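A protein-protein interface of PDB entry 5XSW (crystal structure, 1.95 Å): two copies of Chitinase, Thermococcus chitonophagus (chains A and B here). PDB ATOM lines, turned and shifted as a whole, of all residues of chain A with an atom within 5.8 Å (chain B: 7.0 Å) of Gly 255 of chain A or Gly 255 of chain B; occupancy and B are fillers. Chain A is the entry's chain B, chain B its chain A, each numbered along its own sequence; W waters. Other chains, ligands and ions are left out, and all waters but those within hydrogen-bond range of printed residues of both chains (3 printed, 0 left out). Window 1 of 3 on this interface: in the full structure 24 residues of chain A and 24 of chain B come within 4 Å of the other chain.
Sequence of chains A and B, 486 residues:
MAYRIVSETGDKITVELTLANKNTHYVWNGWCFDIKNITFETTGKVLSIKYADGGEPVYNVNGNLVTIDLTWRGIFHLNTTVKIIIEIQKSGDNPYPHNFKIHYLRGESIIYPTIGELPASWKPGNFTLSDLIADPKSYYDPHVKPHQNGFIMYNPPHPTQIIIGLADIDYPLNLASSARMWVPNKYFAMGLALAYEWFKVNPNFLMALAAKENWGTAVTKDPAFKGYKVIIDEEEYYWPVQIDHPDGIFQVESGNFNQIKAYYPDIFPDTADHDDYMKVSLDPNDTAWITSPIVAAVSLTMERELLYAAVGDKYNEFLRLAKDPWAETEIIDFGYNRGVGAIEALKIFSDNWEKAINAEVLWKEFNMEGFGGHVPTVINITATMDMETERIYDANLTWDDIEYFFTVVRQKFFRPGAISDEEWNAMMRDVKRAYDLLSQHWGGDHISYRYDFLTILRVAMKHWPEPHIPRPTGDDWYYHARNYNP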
ATOM      1  N   GLU A 253      37.731 -17.791  17.527  1.00  0.00           N
ATOM      2  CA  GLU A 253      37.263 -18.199  16.204  1.00  0.00           C
ATOM      3  C   GLU A 253      35.900 -17.676  15.873  1.00  0.00           C
ATOM      4  O   GLU A 253      35.176 -17.235  16.764  1.00  0.00           O
ATOM      5  CB  GLU A 253      37.262 -19.722  16.106  1.00  0.00           C
ATOM      6  CG  GLU A 253      38.691 -20.286  16.230  1.00  0.00           C
ATOM      7  CD  GLU A 253      38.658 -21.832  16.053  1.00  0.00           C
ATOM      8  OE1 GLU A 253      37.852 -22.329  15.263  1.00  0.00           O
ATOM      9  OE2 GLU A 253      39.430 -22.512  16.698  1.00  0.00           O
ATOM     10  N   SER A 254      35.526 -17.734  14.591  1.00  0.00           N
ATOM     11  CA  SER A 254      34.309 -17.059  14.213  1.00  0.00           C
ATOM     12  C   SER A 254      33.076 -17.756  14.786  1.00  0.00           C
ATOM     13  O   SER A 254      32.064 -17.085  15.022  1.00  0.00           O
ATOM     14  CB  SER A 254      34.210 -16.909  12.666  1.00  0.00           C
ATOM     15  OG  SER A 254      34.050 -18.159  12.091  1.00  0.00           O
ATOM     16  N   GLY A 255      33.096 -19.079  14.978  1.00  0.00           N
ATOM     17  CA  GLY A 255      31.921 -19.732  15.511  1.00  0.00           C
ATOM     18  C   GLY A 255      31.644 -19.269  16.985  1.00  0.00           C
ATOM     19  O   GLY A 255      30.526 -18.955  17.332  1.00  0.00           O
ATOM     20  N   ASN A 256      32.675 -19.241  17.826  1.00  0.00           N
ATOM     21  CA  ASN A 256      32.523 -18.747  19.205  1.00  0.00           C
ATOM     22  C   ASN A 256      32.076 -17.264  19.221  1.00  0.00           C
ATOM     23  O   ASN A 256      31.146 -16.882  19.951  1.00  0.00           O
ATOM     24  CB  ASN A 256      33.838 -18.957  19.995  1.00  0.00           C
ATOM     25  CG  ASN A 256      33.741 -18.426  21.483  1.00  0.00           C
ATOM     26  OD1 ASN A 256      34.153 -17.315  21.725  1.00  0.00           O
ATOM     27  ND2 ASN A 256      33.197 -19.223  22.436  1.00  0.00           N
ATOM     28  N   PHE A 257      32.667 -16.457  18.344  1.00  0.00           N
ATOM     29  CA  PHE A 257      32.264 -15.053  18.198  1.00  0.00           C
ATOM     30  C   PHE A 257      30.792 -14.930  17.824  1.00  0.00           C
ATOM     31  O   PHE A 257      30.070 -14.097  18.373  1.00  0.00           O
ATOM     32  CB  PHE A 257      33.132 -14.373  17.124  1.00  0.00           C
ATOM     33  CG  PHE A 257      32.956 -12.904  17.059  1.00  0.00           C
ATOM     34  CD1 PHE A 257      33.670 -12.069  17.927  1.00  0.00           C
ATOM     35  CD2 PHE A 257      32.057 -12.339  16.146  1.00  0.00           C
ATOM     36  CE1 PHE A 257      33.496 -10.642  17.860  1.00  0.00           C
ATOM     37  CE2 PHE A 257      31.897 -10.938  16.083  1.00  0.00           C
ATOM     38  CZ  PHE A 257      32.603 -10.105  16.946  1.00  0.00           C
ATOM     39  N   ASN A 258      30.352 -15.730  16.854  1.00  0.00           N
ATOM     40  CA  ASN A 258      28.921 -15.767  16.445  1.00  0.00           C
ATOM     41  C   ASN A 258      28.001 -16.084  17.646  1.00  0.00           C
ATOM     42  O   ASN A 258      26.945 -15.483  17.858  1.00  0.00           O
ATOM     43  CB  ASN A 258      28.741 -16.870  15.381  1.00  0.00           C
ATOM     44  CG  ASN A 258      27.361 -16.839  14.719  1.00  0.00           C
ATOM     45  OD1 ASN A 258      27.228 -16.372  13.600  1.00  0.00           O
ATOM     46  ND2 ASN A 258      26.340 -17.344  15.419  1.00  0.00           N
ATOM     47  N   GLN A 259      28.439 -17.063  18.413  1.00  0.00           N
ATOM     48  CA  GLN A 259      27.670 -17.494  19.567  1.00  0.00           C
ATOM     49  C   GLN A 259      27.555 -16.388  20.635  1.00  0.00           C
ATOM     50  O   GLN A 259      26.460 -16.181  21.211  1.00  0.00           O
ATOM     51  CB  GLN A 259      28.326 -18.731  20.122  1.00  0.00           C
ATOM     52  CG  GLN A 259      27.622 -19.353  21.280  1.00  0.00           C
ATOM     53  CD  GLN A 259      28.348 -20.563  21.791  1.00  0.00           C
ATOM     54  OE1 GLN A 259      27.767 -21.642  21.858  1.00  0.00           O
ATOM     55  NE2 GLN A 259      29.622 -20.428  22.063  1.00  0.00           N
ATOM     56  N   ILE A 260      28.655 -15.694  20.936  1.00  0.00           N
ATOM     57  CA  ILE A 260      28.531 -14.698  22.004  1.00  0.00           C
ATOM     58  C   ILE A 260      27.788 -13.491  21.530  1.00  0.00           C
ATOM     59  O   ILE A 260      27.144 -12.806  22.361  1.00  0.00           O
ATOM     60  CB  ILE A 260      29.889 -14.304  22.637  1.00  0.00           C
ATOM     61  CG1 ILE A 260      30.859 -13.708  21.651  1.00  0.00           C
ATOM     62  CG2 ILE A 260      30.527 -15.543  23.375  1.00  0.00           C
ATOM     63  CD1 ILE A 260      32.247 -13.653  22.320  1.00  0.00           C
ATOM     64  N   VAL B 252      31.664 -31.745  17.000  1.00  0.00           N
ATOM     65  CA  VAL B 252      31.175 -30.428  16.627  1.00  0.00           C
ATOM     66  C   VAL B 252      30.870 -29.652  17.954  1.00  0.00           C
ATOM     67  O   VAL B 252      30.018 -30.095  18.713  1.00  0.00           O
ATOM     68  CB  VAL B 252      29.868 -30.496  15.787  1.00  0.00           C
ATOM     69  CG1 VAL B 252      29.327 -29.044  15.559  1.00  0.00           C
ATOM     70  CG2 VAL B 252      30.121 -31.229  14.410  1.00  0.00           C
ATOM     71  N   GLU B 253      31.507 -28.504  18.165  1.00  0.00           N
ATOM     72  CA  GLU B 253      31.264 -27.681  19.379  1.00  0.00           C
ATOM     73  C   GLU B 253      30.075 -26.766  19.276  1.00  0.00           C
ATOM     74  O   GLU B 253      29.600 -26.461  18.165  1.00  0.00           O
ATOM     75  CB  GLU B 253      32.531 -26.851  19.680  1.00  0.00           C
ATOM     76  CG  GLU B 253      33.680 -27.781  20.004  1.00  0.00           C
ATOM     77  CD  GLU B 253      34.943 -27.041  20.459  1.00  0.00           C
ATOM     78  OE1 GLU B 253      34.804 -25.979  21.099  1.00  0.00           O
ATOM     79  OE2 GLU B 253      36.059 -27.512  20.159  1.00  0.00           O
ATOM     80  N   SER B 254      29.590 -26.266  20.417  1.00  0.00           N
ATOM     81  CA  SER B 254      28.415 -25.448  20.331  1.00  0.00           C
ATOM     82  C   SER B 254      28.602 -24.119  19.588  1.00  0.00           C
ATOM     83  O   SER B 254      27.631 -23.652  19.016  1.00  0.00           O
ATOM     84  CB  SER B 254      27.797 -25.182  21.731  1.00  0.00           C
ATOM     85  OG  SER B 254      28.603 -24.332  22.489  1.00  0.00           O
ATOM     86  N   GLY B 255      29.785 -23.495  19.593  1.00  0.00           N
ATOM     87  CA  GLY B 255      29.946 -22.219  18.886  1.00  0.00           C
ATOM     88  C   GLY B 255      29.742 -22.450  17.358  1.00  0.00           C
ATOM     89  O   GLY B 255      28.985 -21.740  16.692  1.00  0.00           O
ATOM     90  N   ASN B 256      30.416 -23.452  16.814  1.00  0.00           N
ATOM     91  CA  ASN B 256      30.257 -23.798  15.374  1.00  0.00           C
ATOM     92  C   ASN B 256      28.823 -24.187  15.038  1.00  0.00           C
ATOM     93  O   ASN B 256      28.269 -23.761  14.015  1.00  0.00           O
ATOM     94  CB  ASN B 256      31.222 -24.922  15.008  1.00  0.00           C
ATOM     95  CG  ASN B 256      31.133 -25.307  13.499  1.00  0.00           C
ATOM     96  OD1 ASN B 256      30.485 -26.279  13.176  1.00  0.00           O
ATOM     97  ND2 ASN B 256      31.800 -24.558  12.613  1.00  0.00           N
ATOM     98  N   PHE B 257      28.167 -24.941  15.941  1.00  0.00           N
ATOM     99  CA  PHE B 257      26.739 -25.274  15.758  1.00  0.00           C
ATOM    100  C   PHE B 257      25.873 -24.050  15.714  1.00  0.00           C
ATOM    101  O   PHE B 257      24.951 -23.911  14.869  1.00  0.00           O
ATOM    102  CB  PHE B 257      26.261 -26.223  16.914  1.00  0.00           C
ATOM    103  CG  PHE B 257      24.905 -26.780  16.708  1.00  0.00           C
ATOM    104  CD1 PHE B 257      24.741 -27.967  16.003  1.00  0.00           C
ATOM    105  CD2 PHE B 257      23.776 -26.137  17.240  1.00  0.00           C
ATOM    106  CE1 PHE B 257      23.436 -28.549  15.792  1.00  0.00           C
ATOM    107  CE2 PHE B 257      22.475 -26.683  17.087  1.00  0.00           C
ATOM    108  CZ  PHE B 257      22.278 -27.875  16.336  1.00  0.00           C
ATOM    109  N   ASN B 258      26.100 -23.148  16.668  1.00  0.00           N
ATOM    110  CA  ASN B 258      25.365 -21.886  16.701  1.00  0.00           C
ATOM    111  C   ASN B 258      25.549 -21.096  15.384  1.00  0.00           C
ATOM    112  O   ASN B 258      24.617 -20.525  14.825  1.00  0.00           O
ATOM    113  CB  ASN B 258      25.872 -21.037  17.908  1.00  0.00           C
ATOM    114  CG  ASN B 258      25.150 -19.670  18.036  1.00  0.00           C
ATOM    115  OD1 ASN B 258      25.427 -18.717  17.296  1.00  0.00           O
ATOM    116  ND2 ASN B 258      24.247 -19.576  18.992  1.00  0.00           N
ATOM    117  N   GLN B 259      26.771 -21.071  14.908  1.00  0.00           N
ATOM    118  CA  GLN B 259      27.051 -20.322  13.668  1.00  0.00           C
ATOM    119  C   GLN B 259      26.359 -20.952  12.420  1.00  0.00           C
ATOM    120  O   GLN B 259      25.753 -20.248  11.568  1.00  0.00           O
ATOM    121  CB  GLN B 259      28.573 -20.258  13.500  1.00  0.00           C
ATOM    122  CG  GLN B 259      29.082 -19.663  12.197  1.00  0.00           C
ATOM    123  CD  GLN B 259      30.594 -19.757  12.140  1.00  0.00           C
ATOM    124  OE1 GLN B 259      31.287 -18.741  12.111  1.00  0.00           O
ATOM    125  NE2 GLN B 259      31.100 -20.962  12.233  1.00  0.00           N
ATOM    126  N   ILE B 260      26.403 -22.277  12.287  1.00  0.00           N
ATOM    127  CA  ILE B 260      25.764 -22.848  11.082  1.00  0.00           C
ATOM    128  C   ILE B 260      24.260 -22.818  11.159  1.00  0.00           C
ATOM    129  O   ILE B 260      23.590 -22.617  10.142  1.00  0.00           O
ATOM    130  CB  ILE B 260      26.245 -24.287  10.753  1.00  0.00           C
ATOM    131  CG1 ILE B 260      25.879 -25.274  11.833  1.00  0.00           C
ATOM    132  CG2 ILE B 260      27.751 -24.270  10.441  1.00  0.00           C
ATOM    133  CD1 ILE B 260      26.478 -26.689  11.590  1.00  0.00           C
ATOM    134  N   LYS B 261      23.693 -22.892  12.365  1.00  0.00           N
ATOM    135  CA  LYS B 261      22.298 -22.539  12.545  1.00  0.00           C
ATOM    136  C   LYS B 261      21.979 -21.107  12.063  1.00  0.00           C
ATOM    137  O   LYS B 261      20.960 -20.860  11.371  1.00  0.00           O
ATOM    138  CB  LYS B 261      21.942 -22.702  14.056  1.00  0.00           C
ATOM    139  CG  LYS B 261      20.571 -22.788  14.432  1.00  0.00           C
ATOM    140  CD  LYS B 261      20.487 -23.106  15.988  1.00  0.00           C
ATOM    141  CE  LYS B 261      19.150 -22.595  16.455  1.00  0.00           C
ATOM    142  NZ  LYS B 261      19.069 -22.901  17.916  1.00  0.00           N
ATOM    143  N   TYR B 263      23.603 -19.379   9.830  1.00  0.00           N
ATOM    144  CA  TYR B 263      23.851 -19.286   8.376  1.00  0.00           C
ATOM    145  C   TYR B 263      22.766 -20.002   7.583  1.00  0.00           C
ATOM    146  O   TYR B 263      22.509 -19.697   6.403  1.00  0.00           O
ATOM    147  CB  TYR B 263      25.206 -19.895   8.007  1.00  0.00           C
ATOM    148  CG  TYR B 263      26.431 -19.165   8.495  1.00  0.00           C
ATOM    149  CD1 TYR B 263      26.350 -17.908   9.070  1.00  0.00           C
ATOM    150  CD2 TYR B 263      27.690 -19.774   8.390  1.00  0.00           C
ATOM    151  CE1 TYR B 263      27.501 -17.247   9.541  1.00  0.00           C
ATOM    152  CE2 TYR B 263      28.834 -19.123   8.807  1.00  0.00           C
ATOM    153  CZ  TYR B 263      28.730 -17.859   9.376  1.00  0.00           C
ATOM    154  OH  TYR B 263      29.890 -17.265   9.785  1.00  0.00           O
ATOM    155  N   HIS B 274      22.347 -27.883  20.288  1.00  0.00           N
ATOM    156  CA  HIS B 274      23.612 -28.592  20.051  1.00  0.00           C
ATOM    157  C   HIS B 274      23.666 -30.025  20.616  1.00  0.00           C
ATOM    158  O   HIS B 274      23.916 -31.036  19.882  1.00  0.00           O
ATOM    159  CB  HIS B 274      24.770 -27.766  20.630  1.00  0.00           C
ATOM    160  CG  HIS B 274      26.067 -28.519  20.679  1.00  0.00           C
ATOM    161  ND1 HIS B 274      26.454 -29.276  21.774  1.00  0.00           N
ATOM    162  CD2 HIS B 274      27.037 -28.677  19.757  1.00  0.00           C
ATOM    163  CE1 HIS B 274      27.607 -29.866  21.514  1.00  0.00           C
ATOM    164  NE2 HIS B 274      28.011 -29.476  20.316  1.00  0.00           N
ATOM    165  N   VAL B 340      37.924 -21.667  10.088  1.00  0.00           N
ATOM    166  CA  VAL B 340      38.106 -20.955   8.802  1.00  0.00           C
ATOM    167  C   VAL B 340      39.057 -19.763   8.917  1.00  0.00           C
ATOM    168  O   VAL B 340      39.608 -19.293   7.888  1.00  0.00           O
ATOM    169  CB  VAL B 340      36.743 -20.484   8.221  1.00  0.00           C
ATOM    170  CG1 VAL B 340      35.838 -21.675   7.938  1.00  0.00           C
ATOM    171  CG2 VAL B 340      36.034 -19.485   9.175  1.00  0.00           C
ATOM    172  N   HIS B 480      30.584 -11.788   7.854  1.00  0.00           N
ATOM    173  CA  HIS B 480      31.715 -12.696   7.846  1.00  0.00           C
ATOM    174  C   HIS B 480      32.249 -12.946   6.409  1.00  0.00           C
ATOM    175  O   HIS B 480      33.435 -12.832   6.130  1.00  0.00           O
ATOM    176  CB  HIS B 480      31.318 -14.049   8.447  1.00  0.00           C
ATOM    177  CG  HIS B 480      32.491 -14.929   8.708  1.00  0.00           C
ATOM    178  ND1 HIS B 480      32.413 -16.304   8.702  1.00  0.00           N
ATOM    179  CD2 HIS B 480      33.761 -14.622   9.052  1.00  0.00           C
ATOM    180  CE1 HIS B 480      33.599 -16.809   8.994  1.00  0.00           C
ATOM    181  NE2 HIS B 480      34.446 -15.804   9.175  1.00  0.00           N
HETATM  182  O   HOH W   1      24.385 -21.977  21.181  1.00  0.00           O
HETATM  183  O   HOH W   2      37.482 -19.685  12.672  1.00  0.00           O
HETATM  184  O   HOH W   3      29.778 -15.626  11.964  1.00  0.00           O
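Hydrophobic or aromatic side chains of chain B within 4 Å of the printed part of chain A: Val 340 and His 480.
Along chain A the printed residues that touch a printed residue of chain B span positions 254 to 259.
Among the printed residues, no Asp or Glu carboxylate lies within 4 Å of a Lys or Arg side-chain nitrogen of the other chain.
Among the printed residues, merely in contact across the chains: Ser 254 of chain A with Val 340 of chain B, Ser 254 of chain A with His 480 of chain B, Asn 258 of chain A with Gln 259 of chain B, Gln 259 of chain A with Gly 255 of chain B and Gln 259 of chain A with Asn 258 of chain B.
The backbone carbonyl oxygen (O) of Gly 255 of chain A lies close to the backbone carbonyl oxygen (O) of Gly 255 of chain B, at 3.2 Å.
OG of Ser 254 of chain B lies within hydrogen-bond range of OE1 of Gln 259 of chain A, at 2.9 Å.
ND2 of Asn 258 of chain A sits at hydrogen-bond distance from OD1 of Asn 258 of chain B (2.5 Å).
N of Gly 255 of chain A sits at hydrogen-bond distance from OE1 of Gln 259 of chain B (3.4 Å).
OG of Ser 254 of chain A is in hydrogen-bond range of OE1 of Gln 259 of chain B, 2.8 Å away.
Water W3 lies within hydrogen-bond range of OH of Tyr 263 of chain B (2.7 Å), OD1 of Asn 258 of chain A (3.1 Å) and OE1 of Gln 259 of chain B (3.5 Å).
Water W1 lies within hydrogen-bond range of the side-chain amide nitrogen of Asn 258 of chain B and the side-chain amide oxygen of Gln 259 of chain A.
Water W2 lies within hydrogen-bond range of the backbone NH of Val 340 of chain B and the backbone NH of Ser 254 of chain A.
Gly 255 of chain A touches just these residues of chain B: Gly 255 (3.2 Å) and Gln 259 (3.4 Å).
Gly 255 of chain B touches just these residues of chain A: Gly 255 and Gln 259.
Of the printed residues of chain A, Val 340 of chain B touches Ser 254 (3.8 Å).
Of the printed residues of chain A, Gln 259 of chain B touches Ser 254, Gly 255 and Asn 258.
Tyr 263 of chain B touches none of the printed residues of chain A.
The nearest residue of chain B that does not touch Gly 255 of chain A is Asn 256 of chain B (4.2 Å).
The nearest residue of chain A that does not touch Gly 255 of chain B is Asn 256 of chain A (4.2 Å).
The nearest printed residue of chain A that does not touch His 480 of chain B is Gly 255 of chain A (6.4 Å).
A ring nitrogen (ND1) of His 480 of chain B is in hydrogen-bond range of the side-chain hydroxyl (OH) of Tyr 263 of chain B, 2.9 Å away.
The side-chain hydroxyl (OH) of Tyr 263 of chain B lies within hydrogen-bond range of the side-chain amide oxygen (OE1) of Gln 259 of chain B.
Ser 254 of chain A touches Gln 259 of chain B, and with the chains exchanged Gln 259 of chain A touches Ser 254 of chain B.
Gly 255 of chain B touches its own counterpart, Gly 255 of chain A.
Asn 258 of chain A touches its own counterpart, Asn 258 of chain B.
Asn 258 of chain A touches Gln 259 of chain B, and with the chains exchanged Gln 259 of chain A touches Asn 258 of chain B.
Positions printed for both chains: 253, 254, 255, 256, 257, 258, 259 and 260.
Of the 10 pairs that touch across the chains among the printed residues, 8 have their exchanged pair printed and touching as well.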
